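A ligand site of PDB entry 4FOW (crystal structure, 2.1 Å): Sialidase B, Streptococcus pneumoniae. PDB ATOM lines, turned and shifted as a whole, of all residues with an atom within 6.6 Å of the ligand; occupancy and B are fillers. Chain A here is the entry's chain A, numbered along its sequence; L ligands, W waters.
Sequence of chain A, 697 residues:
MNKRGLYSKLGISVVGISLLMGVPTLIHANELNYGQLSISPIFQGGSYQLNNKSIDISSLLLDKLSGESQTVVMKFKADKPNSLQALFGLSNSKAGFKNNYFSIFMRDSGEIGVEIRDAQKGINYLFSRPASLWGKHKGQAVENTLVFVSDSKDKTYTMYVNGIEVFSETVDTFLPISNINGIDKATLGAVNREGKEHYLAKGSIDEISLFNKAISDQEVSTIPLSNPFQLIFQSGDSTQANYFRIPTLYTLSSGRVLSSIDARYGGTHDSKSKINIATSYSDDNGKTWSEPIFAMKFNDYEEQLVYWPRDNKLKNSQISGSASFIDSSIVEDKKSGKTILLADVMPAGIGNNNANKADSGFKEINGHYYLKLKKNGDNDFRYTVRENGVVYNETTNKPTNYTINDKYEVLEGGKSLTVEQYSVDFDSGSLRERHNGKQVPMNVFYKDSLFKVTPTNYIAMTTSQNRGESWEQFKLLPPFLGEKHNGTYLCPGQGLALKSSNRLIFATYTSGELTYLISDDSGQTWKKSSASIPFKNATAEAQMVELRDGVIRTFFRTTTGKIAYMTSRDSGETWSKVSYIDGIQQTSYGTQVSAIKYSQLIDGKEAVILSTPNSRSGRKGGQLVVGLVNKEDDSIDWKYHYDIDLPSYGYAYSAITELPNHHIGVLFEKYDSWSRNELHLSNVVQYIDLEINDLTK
Merely in contact with the ligand: Asp 270 and Trp 674. Hydrophobic or aromatic side chains that line the ligand: Trp 674. The nearest printed residue that does not touch the ligand is Thr 539 (4.2 Å).
Water W2 lies within hydrogen-bond range of OD1 of Asp 327 (2.7 Å), N1 of the ligand (2.7 Å), NH2 of Arg 264 (3.0 Å) and OD1 of Asp 270 (3.1 Å). Water W1 lies within hydrogen-bond range of OD2 of Asp 270 (2.7 Å) and O2 of the ligand (2.8 Å).
N1 of the ligand lies within salt-bridge range of OE1 of Glu 541 (2.8 Å). N1 of the ligand lies within hydrogen-bond range of OH of Tyr 653, 3.3 Å away. An oxygen (O1) of the ligand is in salt-bridge range of the guanidinium group (NH1) of Arg 245, at 3.0 Å. The guanidinium group (NH2) of Arg 619 lies within salt-bridge range of an oxygen (O3) of the ligand (2.8 Å). The side-chain carboxylate of Asp 327 lies within salt-bridge range of a nitrogen (N1) of the ligand, 3.0 Å away. An oxygen (O3) of the ligand is in salt-bridge range of the guanidinium group (NH1) of Arg 557 (3.0 Å).
NH1 of Arg 245 lies within salt-bridge range of OD2 of Asp 270, at 3.7 Å. The backbone carbonyl oxygen of Gly 590 lies within hydrogen-bond range of the guanidinium group of Arg 557 (3.3 Å). The side-chain hydroxyl (OG) of Ser 673 sits at hydrogen-bond distance from the guanidinium group (NH2) of Arg 245 (3.2 Å). The guanidinium group of Arg 557 lies within hydrogen-bond range of the side-chain hydroxyl of Tyr 653 (2.8 Å). The backbone carbonyl oxygen (O) of Tyr 653 is in hydrogen-bond range of the backbone NH (N) of Glu 669 (3.0 Å). The guanidinium group (NH1) of Arg 619 lies within hydrogen-bond range of the side-chain hydroxyl (OG) of Ser 673, 2.9 Å away. The guanidinium group of Arg 557 is in hydrogen-bond range of the backbone carbonyl oxygen of Tyr 589, at 2.9 Å. The guanidinium group (NH2) of Arg 619 sits at hydrogen-bond distance from the backbone carbonyl oxygen (O) of Gly 590 (3.0 Å).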
ATOM      1  N   ARG A 245     -16.952 -26.701 -11.254  1.00  0.00           N
ATOM      2  CA  ARG A 245     -18.140 -26.350 -10.516  1.00  0.00           C
ATOM      3  C   ARG A 245     -19.328 -26.982 -11.213  1.00  0.00           C
ATOM      4  O   ARG A 245     -19.224 -27.402 -12.385  1.00  0.00           O
ATOM      5  CB  ARG A 245     -18.313 -24.822 -10.471  1.00  0.00           C
ATOM      6  CG  ARG A 245     -17.564 -24.086  -9.345  1.00  0.00           C
ATOM      7  CD  ARG A 245     -18.356 -22.808  -8.890  1.00  0.00           C
ATOM      8  NE  ARG A 245     -19.689 -23.143  -8.375  1.00  0.00           N
ATOM      9  CZ  ARG A 245     -20.643 -22.257  -8.104  1.00  0.00           C
ATOM     10  NH1 ARG A 245     -20.433 -20.956  -8.275  1.00  0.00           N
ATOM     11  NH2 ARG A 245     -21.818 -22.681  -7.637  1.00  0.00           N
ATOM     12  N   ILE A 246     -20.458 -27.025 -10.527  1.00  0.00           N
ATOM     13  CA  ILE A 246     -21.726 -27.490 -11.109  1.00  0.00           C
ATOM     14  C   ILE A 246     -21.720 -28.974 -11.509  1.00  0.00           C
ATOM     15  O   ILE A 246     -21.872 -29.302 -12.688  1.00  0.00           O
ATOM     16  CB  ILE A 246     -22.168 -26.607 -12.295  1.00  0.00           C
ATOM     17  CG1 ILE A 246     -21.759 -25.128 -12.103  1.00  0.00           C
ATOM     18  CG2 ILE A 246     -23.667 -26.675 -12.455  1.00  0.00           C
ATOM     19  CD1 ILE A 246     -22.542 -24.407 -10.992  1.00  0.00           C
ATOM     20  N   ARG A 264     -13.860 -25.307 -15.471  1.00  0.00           N
ATOM     21  CA  ARG A 264     -13.666 -23.857 -15.499  1.00  0.00           C
ATOM     22  C   ARG A 264     -12.200 -23.474 -15.477  1.00  0.00           C
ATOM     23  O   ARG A 264     -11.436 -23.847 -14.581  1.00  0.00           O
ATOM     24  CB  ARG A 264     -14.433 -23.192 -14.349  1.00  0.00           C
ATOM     25  CG  ARG A 264     -15.932 -23.498 -14.353  1.00  0.00           C
ATOM     26  CD  ARG A 264     -16.696 -22.591 -13.401  1.00  0.00           C
ATOM     27  NE  ARG A 264     -18.146 -22.742 -13.530  1.00  0.00           N
ATOM     28  CZ  ARG A 264     -19.030 -21.946 -12.910  1.00  0.00           C
ATOM     29  NH1 ARG A 264     -18.604 -20.974 -12.108  1.00  0.00           N
ATOM     30  NH2 ARG A 264     -20.325 -22.139 -13.070  1.00  0.00           N
ATOM     31  N   ASP A 270     -18.231 -17.699 -12.611  1.00  0.00           N
ATOM     32  CA  ASP A 270     -19.237 -17.963 -13.644  1.00  0.00           C
ATOM     33  C   ASP A 270     -18.852 -17.175 -14.897  1.00  0.00           C
ATOM     34  O   ASP A 270     -18.033 -16.251 -14.833  1.00  0.00           O
ATOM     35  CB  ASP A 270     -20.623 -17.471 -13.213  1.00  0.00           C
ATOM     36  CG  ASP A 270     -21.277 -18.384 -12.191  1.00  0.00           C
ATOM     37  OD1 ASP A 270     -22.536 -18.464 -12.217  1.00  0.00           O
ATOM     38  OD2 ASP A 270     -20.572 -18.996 -11.351  1.00  0.00           O
ATOM     39  N   ILE A 326     -21.989 -23.313 -19.609  1.00  0.00           N
ATOM     40  CA  ILE A 326     -22.120 -23.233 -18.149  1.00  0.00           C
ATOM     41  C   ILE A 326     -23.448 -23.833 -17.724  1.00  0.00           C
ATOM     42  O   ILE A 326     -24.428 -23.686 -18.444  1.00  0.00           O
ATOM     43  CB  ILE A 326     -21.968 -21.761 -17.655  1.00  0.00           C
ATOM     44  CG1 ILE A 326     -22.155 -21.659 -16.149  1.00  0.00           C
ATOM     45  CG2 ILE A 326     -22.956 -20.826 -18.379  1.00  0.00           C
ATOM     46  CD1 ILE A 326     -21.807 -20.232 -15.616  1.00  0.00           C
ATOM     47  N   ASP A 327     -23.458 -24.518 -16.572  1.00  0.00           N
ATOM     48  CA  ASP A 327     -24.649 -25.163 -16.027  1.00  0.00           C
ATOM     49  C   ASP A 327     -25.185 -26.285 -16.935  1.00  0.00           C
ATOM     50  O   ASP A 327     -26.013 -26.039 -17.813  1.00  0.00           O
ATOM     51  CB  ASP A 327     -25.767 -24.141 -15.749  1.00  0.00           C
ATOM     52  CG  ASP A 327     -25.403 -23.141 -14.654  1.00  0.00           C
ATOM     53  OD1 ASP A 327     -24.335 -23.275 -14.011  1.00  0.00           O
ATOM     54  OD2 ASP A 327     -26.215 -22.208 -14.428  1.00  0.00           O
ATOM     55  N   ASP A 344     -26.153 -24.091 -20.826  1.00  0.00           N
ATOM     56  CA  ASP A 344     -26.228 -22.717 -21.336  1.00  0.00           C
ATOM     57  C   ASP A 344     -25.010 -22.476 -22.231  1.00  0.00           C
ATOM     58  O   ASP A 344     -23.930 -23.011 -21.951  1.00  0.00           O
ATOM     59  CB  ASP A 344     -26.196 -21.693 -20.189  1.00  0.00           C
ATOM     60  CG  ASP A 344     -27.341 -21.863 -19.185  1.00  0.00           C
ATOM     61  OD1 ASP A 344     -28.433 -22.347 -19.567  1.00  0.00           O
ATOM     62  OD2 ASP A 344     -27.171 -21.456 -18.014  1.00  0.00           O
ATOM     63  N   LEU A 490     -30.911 -22.898 -17.888  1.00  0.00           N
ATOM     64  CA  LEU A 490     -31.037 -24.319 -17.577  1.00  0.00           C
ATOM     65  C   LEU A 490     -30.823 -24.564 -16.101  1.00  0.00           C
ATOM     66  O   LEU A 490     -29.906 -24.004 -15.490  1.00  0.00           O
ATOM     67  CB  LEU A 490     -30.003 -25.107 -18.368  1.00  0.00           C
ATOM     68  CG  LEU A 490     -30.140 -26.623 -18.266  1.00  0.00           C
ATOM     69  CD1 LEU A 490     -31.432 -27.049 -18.932  1.00  0.00           C
ATOM     70  CD2 LEU A 490     -28.951 -27.278 -18.930  1.00  0.00           C
ATOM     71  N   PRO A 492     -29.264 -26.769 -13.485  1.00  0.00           N
ATOM     72  CA  PRO A 492     -28.207 -27.772 -13.506  1.00  0.00           C
ATOM     73  C   PRO A 492     -28.626 -29.022 -12.747  1.00  0.00           C
ATOM     74  O   PRO A 492     -29.336 -28.921 -11.738  1.00  0.00           O
ATOM     75  CB  PRO A 492     -27.050 -27.113 -12.742  1.00  0.00           C
ATOM     76  CG  PRO A 492     -27.454 -25.665 -12.516  1.00  0.00           C
ATOM     77  CD  PRO A 492     -28.945 -25.615 -12.616  1.00  0.00           C
ATOM     78  N   TYR A 509     -35.413 -21.757 -15.849  1.00  0.00           N
ATOM     79  CA  TYR A 509     -36.097 -20.638 -15.204  1.00  0.00           C
ATOM     80  C   TYR A 509     -35.794 -19.307 -15.882  1.00  0.00           C
ATOM     81  O   TYR A 509     -34.785 -19.154 -16.601  1.00  0.00           O
ATOM     82  CB  TYR A 509     -35.727 -20.563 -13.731  1.00  0.00           C
ATOM     83  CG  TYR A 509     -34.271 -20.209 -13.487  1.00  0.00           C
ATOM     84  CD1 TYR A 509     -33.889 -18.899 -13.212  1.00  0.00           C
ATOM     85  CD2 TYR A 509     -33.289 -21.185 -13.535  1.00  0.00           C
ATOM     86  CE1 TYR A 509     -32.554 -18.577 -12.988  1.00  0.00           C
ATOM     87  CE2 TYR A 509     -31.965 -20.884 -13.312  1.00  0.00           C
ATOM     88  CZ  TYR A 509     -31.602 -19.574 -13.043  1.00  0.00           C
ATOM     89  OH  TYR A 509     -30.274 -19.289 -12.836  1.00  0.00           O
ATOM     90  N   THR A 539     -32.834 -16.890  -8.846  1.00  0.00           N
ATOM     91  CA  THR A 539     -32.052 -17.952  -9.457  1.00  0.00           C
ATOM     92  C   THR A 539     -32.773 -19.224  -9.070  1.00  0.00           C
ATOM     93  O   THR A 539     -32.348 -19.942  -8.164  1.00  0.00           O
ATOM     94  CB  THR A 539     -30.599 -17.933  -8.904  1.00  0.00           C
ATOM     95  OG1 THR A 539     -30.032 -16.642  -9.136  1.00  0.00           O
ATOM     96  CG2 THR A 539     -29.700 -18.984  -9.584  1.00  0.00           C
ATOM     97  N   GLU A 541     -33.232 -22.345  -9.449  1.00  0.00           N
ATOM     98  CA  GLU A 541     -32.727 -23.642  -9.897  1.00  0.00           C
ATOM     99  C   GLU A 541     -33.601 -24.764  -9.335  1.00  0.00           C
ATOM    100  O   GLU A 541     -33.739 -24.895  -8.117  1.00  0.00           O
ATOM    101  CB  GLU A 541     -31.261 -23.809  -9.479  1.00  0.00           C
ATOM    102  CG  GLU A 541     -30.312 -22.975 -10.350  1.00  0.00           C
ATOM    103  CD  GLU A 541     -28.985 -22.664  -9.684  1.00  0.00           C
ATOM    104  OE1 GLU A 541     -28.039 -22.252 -10.392  1.00  0.00           O
ATOM    105  OE2 GLU A 541     -28.869 -22.810  -8.439  1.00  0.00           O
ATOM    106  N   ARG A 557     -34.761 -23.594  -5.684  1.00  0.00           N
ATOM    107  CA  ARG A 557     -34.087 -22.518  -4.948  1.00  0.00           C
ATOM    108  C   ARG A 557     -34.905 -21.249  -5.035  1.00  0.00           C
ATOM    109  O   ARG A 557     -35.562 -20.995  -6.052  1.00  0.00           O
ATOM    110  CB  ARG A 557     -32.722 -22.286  -5.615  1.00  0.00           C
ATOM    111  CG  ARG A 557     -31.909 -21.111  -5.131  1.00  0.00           C
ATOM    112  CD  ARG A 557     -30.591 -21.086  -5.883  1.00  0.00           C
ATOM    113  NE  ARG A 557     -29.833 -19.857  -5.644  1.00  0.00           N
ATOM    114  CZ  ARG A 557     -28.612 -19.637  -6.129  1.00  0.00           C
ATOM    115  NH1 ARG A 557     -28.020 -20.564  -6.878  1.00  0.00           N
ATOM    116  NH2 ARG A 557     -28.004 -18.491  -5.862  1.00  0.00           N
ATOM    117  N   TYR A 589     -29.757 -15.807  -0.639  1.00  0.00           N
ATOM    118  CA  TYR A 589     -29.468 -15.939  -2.076  1.00  0.00           C
ATOM    119  C   TYR A 589     -29.686 -17.366  -2.587  1.00  0.00           C
ATOM    120  O   TYR A 589     -29.920 -17.585  -3.787  1.00  0.00           O
ATOM    121  CB  TYR A 589     -28.041 -15.465  -2.404  1.00  0.00           C
ATOM    122  CG  TYR A 589     -26.968 -16.046  -1.526  1.00  0.00           C
ATOM    123  CD1 TYR A 589     -26.440 -17.318  -1.777  1.00  0.00           C
ATOM    124  CD2 TYR A 589     -26.458 -15.330  -0.445  1.00  0.00           C
ATOM    125  CE1 TYR A 589     -25.460 -17.862  -0.962  1.00  0.00           C
ATOM    126  CE2 TYR A 589     -25.469 -15.865   0.377  1.00  0.00           C
ATOM    127  CZ  TYR A 589     -24.976 -17.131   0.105  1.00  0.00           C
ATOM    128  OH  TYR A 589     -24.000 -17.667   0.899  1.00  0.00           O
ATOM    129  N   GLY A 590     -29.610 -18.329  -1.682  1.00  0.00           N
ATOM    130  CA  GLY A 590     -29.995 -19.700  -1.993  1.00  0.00           C
ATOM    131  C   GLY A 590     -28.882 -20.524  -2.613  1.00  0.00           C
ATOM    132  O   GLY A 590     -27.822 -19.999  -2.969  1.00  0.00           O
ATOM    133  N   THR A 591     -29.136 -21.830  -2.730  1.00  0.00           N
ATOM    134  CA  THR A 591     -28.207 -22.761  -3.353  1.00  0.00           C
ATOM    135  C   THR A 591     -29.030 -23.827  -4.080  1.00  0.00           C
ATOM    136  O   THR A 591     -30.138 -24.183  -3.642  1.00  0.00           O
ATOM    137  CB  THR A 591     -27.302 -23.469  -2.301  1.00  0.00           C
ATOM    138  OG1 THR A 591     -26.650 -22.488  -1.485  1.00  0.00           O
ATOM    139  CG2 THR A 591     -26.234 -24.327  -2.983  1.00  0.00           C
ATOM    140  N   GLN A 592     -28.488 -24.328  -5.189  1.00  0.00           N
ATOM    141  CA  GLN A 592     -29.074 -25.446  -5.911  1.00  0.00           C
ATOM    142  C   GLN A 592     -29.381 -26.589  -4.959  1.00  0.00           C
ATOM    143  O   GLN A 592     -28.642 -26.837  -4.001  1.00  0.00           O
ATOM    144  CB  GLN A 592     -28.104 -25.896  -6.999  1.00  0.00           C
ATOM    145  CG  GLN A 592     -28.601 -27.038  -7.902  1.00  0.00           C
ATOM    146  CD  GLN A 592     -27.590 -28.165  -7.998  1.00  0.00           C
ATOM    147  OE1 GLN A 592     -26.662 -28.247  -7.203  1.00  0.00           O
ATOM    148  NE2 GLN A 592     -27.778 -29.042  -8.963  1.00  0.00           N
ATOM    149  N   ARG A 619     -22.971 -21.328   2.502  1.00  0.00           N
ATOM    150  CA  ARG A 619     -23.100 -22.628   1.834  1.00  0.00           C
ATOM    151  C   ARG A 619     -22.241 -23.636   2.586  1.00  0.00           C
ATOM    152  O   ARG A 619     -21.073 -23.879   2.254  1.00  0.00           O
ATOM    153  CB  ARG A 619     -22.688 -22.523   0.351  1.00  0.00           C
ATOM    154  CG  ARG A 619     -23.608 -21.605  -0.457  1.00  0.00           C
ATOM    155  CD  ARG A 619     -23.288 -21.593  -1.963  1.00  0.00           C
ATOM    156  NE  ARG A 619     -24.402 -21.045  -2.755  1.00  0.00           N
ATOM    157  CZ  ARG A 619     -24.296 -20.672  -4.027  1.00  0.00           C
ATOM    158  NH1 ARG A 619     -23.130 -20.785  -4.659  1.00  0.00           N
ATOM    159  NH2 ARG A 619     -25.354 -20.183  -4.676  1.00  0.00           N
ATOM    160  N   TYR A 653     -23.236 -26.506  -4.419  1.00  0.00           N
ATOM    161  CA  TYR A 653     -23.971 -27.239  -5.461  1.00  0.00           C
ATOM    162  C   TYR A 653     -23.733 -28.729  -5.310  1.00  0.00           C
ATOM    163  O   TYR A 653     -22.661 -29.147  -4.854  1.00  0.00           O
ATOM    164  CB  TYR A 653     -23.566 -26.760  -6.859  1.00  0.00           C
ATOM    165  CG  TYR A 653     -24.309 -25.522  -7.314  1.00  0.00           C
ATOM    166  CD1 TYR A 653     -24.415 -24.407  -6.472  1.00  0.00           C
ATOM    167  CD2 TYR A 653     -24.899 -25.445  -8.568  1.00  0.00           C
ATOM    168  CE1 TYR A 653     -25.096 -23.260  -6.873  1.00  0.00           C
ATOM    169  CE2 TYR A 653     -25.576 -24.304  -8.982  1.00  0.00           C
ATOM    170  CZ  TYR A 653     -25.675 -23.211  -8.134  1.00  0.00           C
ATOM    171  OH  TYR A 653     -26.345 -22.074  -8.536  1.00  0.00           O
ATOM    172  N   GLU A 669     -19.771 -29.730  -4.420  1.00  0.00           N
ATOM    173  CA  GLU A 669     -18.806 -28.686  -4.136  1.00  0.00           C
ATOM    174  C   GLU A 669     -18.552 -28.649  -2.639  1.00  0.00           C
ATOM    175  O   GLU A 669     -19.402 -28.177  -1.884  1.00  0.00           O
ATOM    176  CB  GLU A 669     -19.352 -27.338  -4.628  1.00  0.00           C
ATOM    177  CG  GLU A 669     -19.463 -27.228  -6.154  1.00  0.00           C
ATOM    178  CD  GLU A 669     -20.191 -25.965  -6.617  1.00  0.00           C
ATOM    179  OE1 GLU A 669     -20.702 -25.192  -5.753  1.00  0.00           O
ATOM    180  OE2 GLU A 669     -20.277 -25.739  -7.843  1.00  0.00           O
ATOM    181  N   SER A 673     -19.101 -21.887  -2.367  1.00  0.00           N
ATOM    182  CA  SER A 673     -18.900 -21.345  -3.709  1.00  0.00           C
ATOM    183  C   SER A 673     -19.571 -19.973  -3.875  1.00  0.00           C
ATOM    184  O   SER A 673     -19.553 -19.392  -4.973  1.00  0.00           O
ATOM    185  CB  SER A 673     -19.411 -22.324  -4.769  1.00  0.00           C
ATOM    186  OG  SER A 673     -20.792 -22.577  -4.576  1.00  0.00           O
ATOM    187  N   TRP A 674     -20.140 -19.437  -2.807  1.00  0.00           N
ATOM    188  CA  TRP A 674     -20.627 -18.054  -2.825  1.00  0.00           C
ATOM    189  C   TRP A 674     -19.544 -17.121  -2.274  1.00  0.00           C
ATOM    190  O   TRP A 674     -19.311 -16.028  -2.808  1.00  0.00           O
ATOM    191  CB  TRP A 674     -21.930 -17.905  -2.024  1.00  0.00           C
ATOM    192  CG  TRP A 674     -22.588 -16.551  -2.169  1.00  0.00           C
ATOM    193  CD1 TRP A 674     -22.446 -15.454  -1.349  1.00  0.00           C
ATOM    194  CD2 TRP A 674     -23.491 -16.143  -3.213  1.00  0.00           C
ATOM    195  NE1 TRP A 674     -23.215 -14.405  -1.819  1.00  0.00           N
ATOM    196  CE2 TRP A 674     -23.858 -14.799  -2.957  1.00  0.00           C
ATOM    197  CE3 TRP A 674     -24.037 -16.793  -4.337  1.00  0.00           C
ATOM    198  CZ2 TRP A 674     -24.743 -14.098  -3.780  1.00  0.00           C
ATOM    199  CZ3 TRP A 674     -24.912 -16.092  -5.156  1.00  0.00           C
ATOM    200  CH2 TRP A 674     -25.256 -14.756  -4.874  1.00  0.00           C
HETATM  201  O1  LIG L   1     -23.077 -19.804  -7.325  1.00  0.00           O
HETATM  202  S1  LIG L   1     -24.122 -19.038  -8.032  1.00  0.00           S
HETATM  203  O2  LIG L   1     -23.705 -17.639  -8.172  1.00  0.00           O
HETATM  204  O3  LIG L   1     -25.385 -19.138  -7.267  1.00  0.00           O
HETATM  205  C1  LIG L   1     -24.323 -19.734  -9.641  1.00  0.00           C
HETATM  206  C2  LIG L   1     -25.585 -19.231 -10.276  1.00  0.00           C
HETATM  207  C3  LIG L   1     -25.715 -19.782 -11.658  1.00  0.00           C
HETATM  208  N1  LIG L   1     -25.691 -21.223 -11.618  1.00  0.00           N
HETATM  209  O   HOH W   1     -21.084 -17.592  -9.141  1.00  0.00           O
HETATM  210  O   HOH W   2     -23.125 -21.459 -12.434  1.00  0.00           O
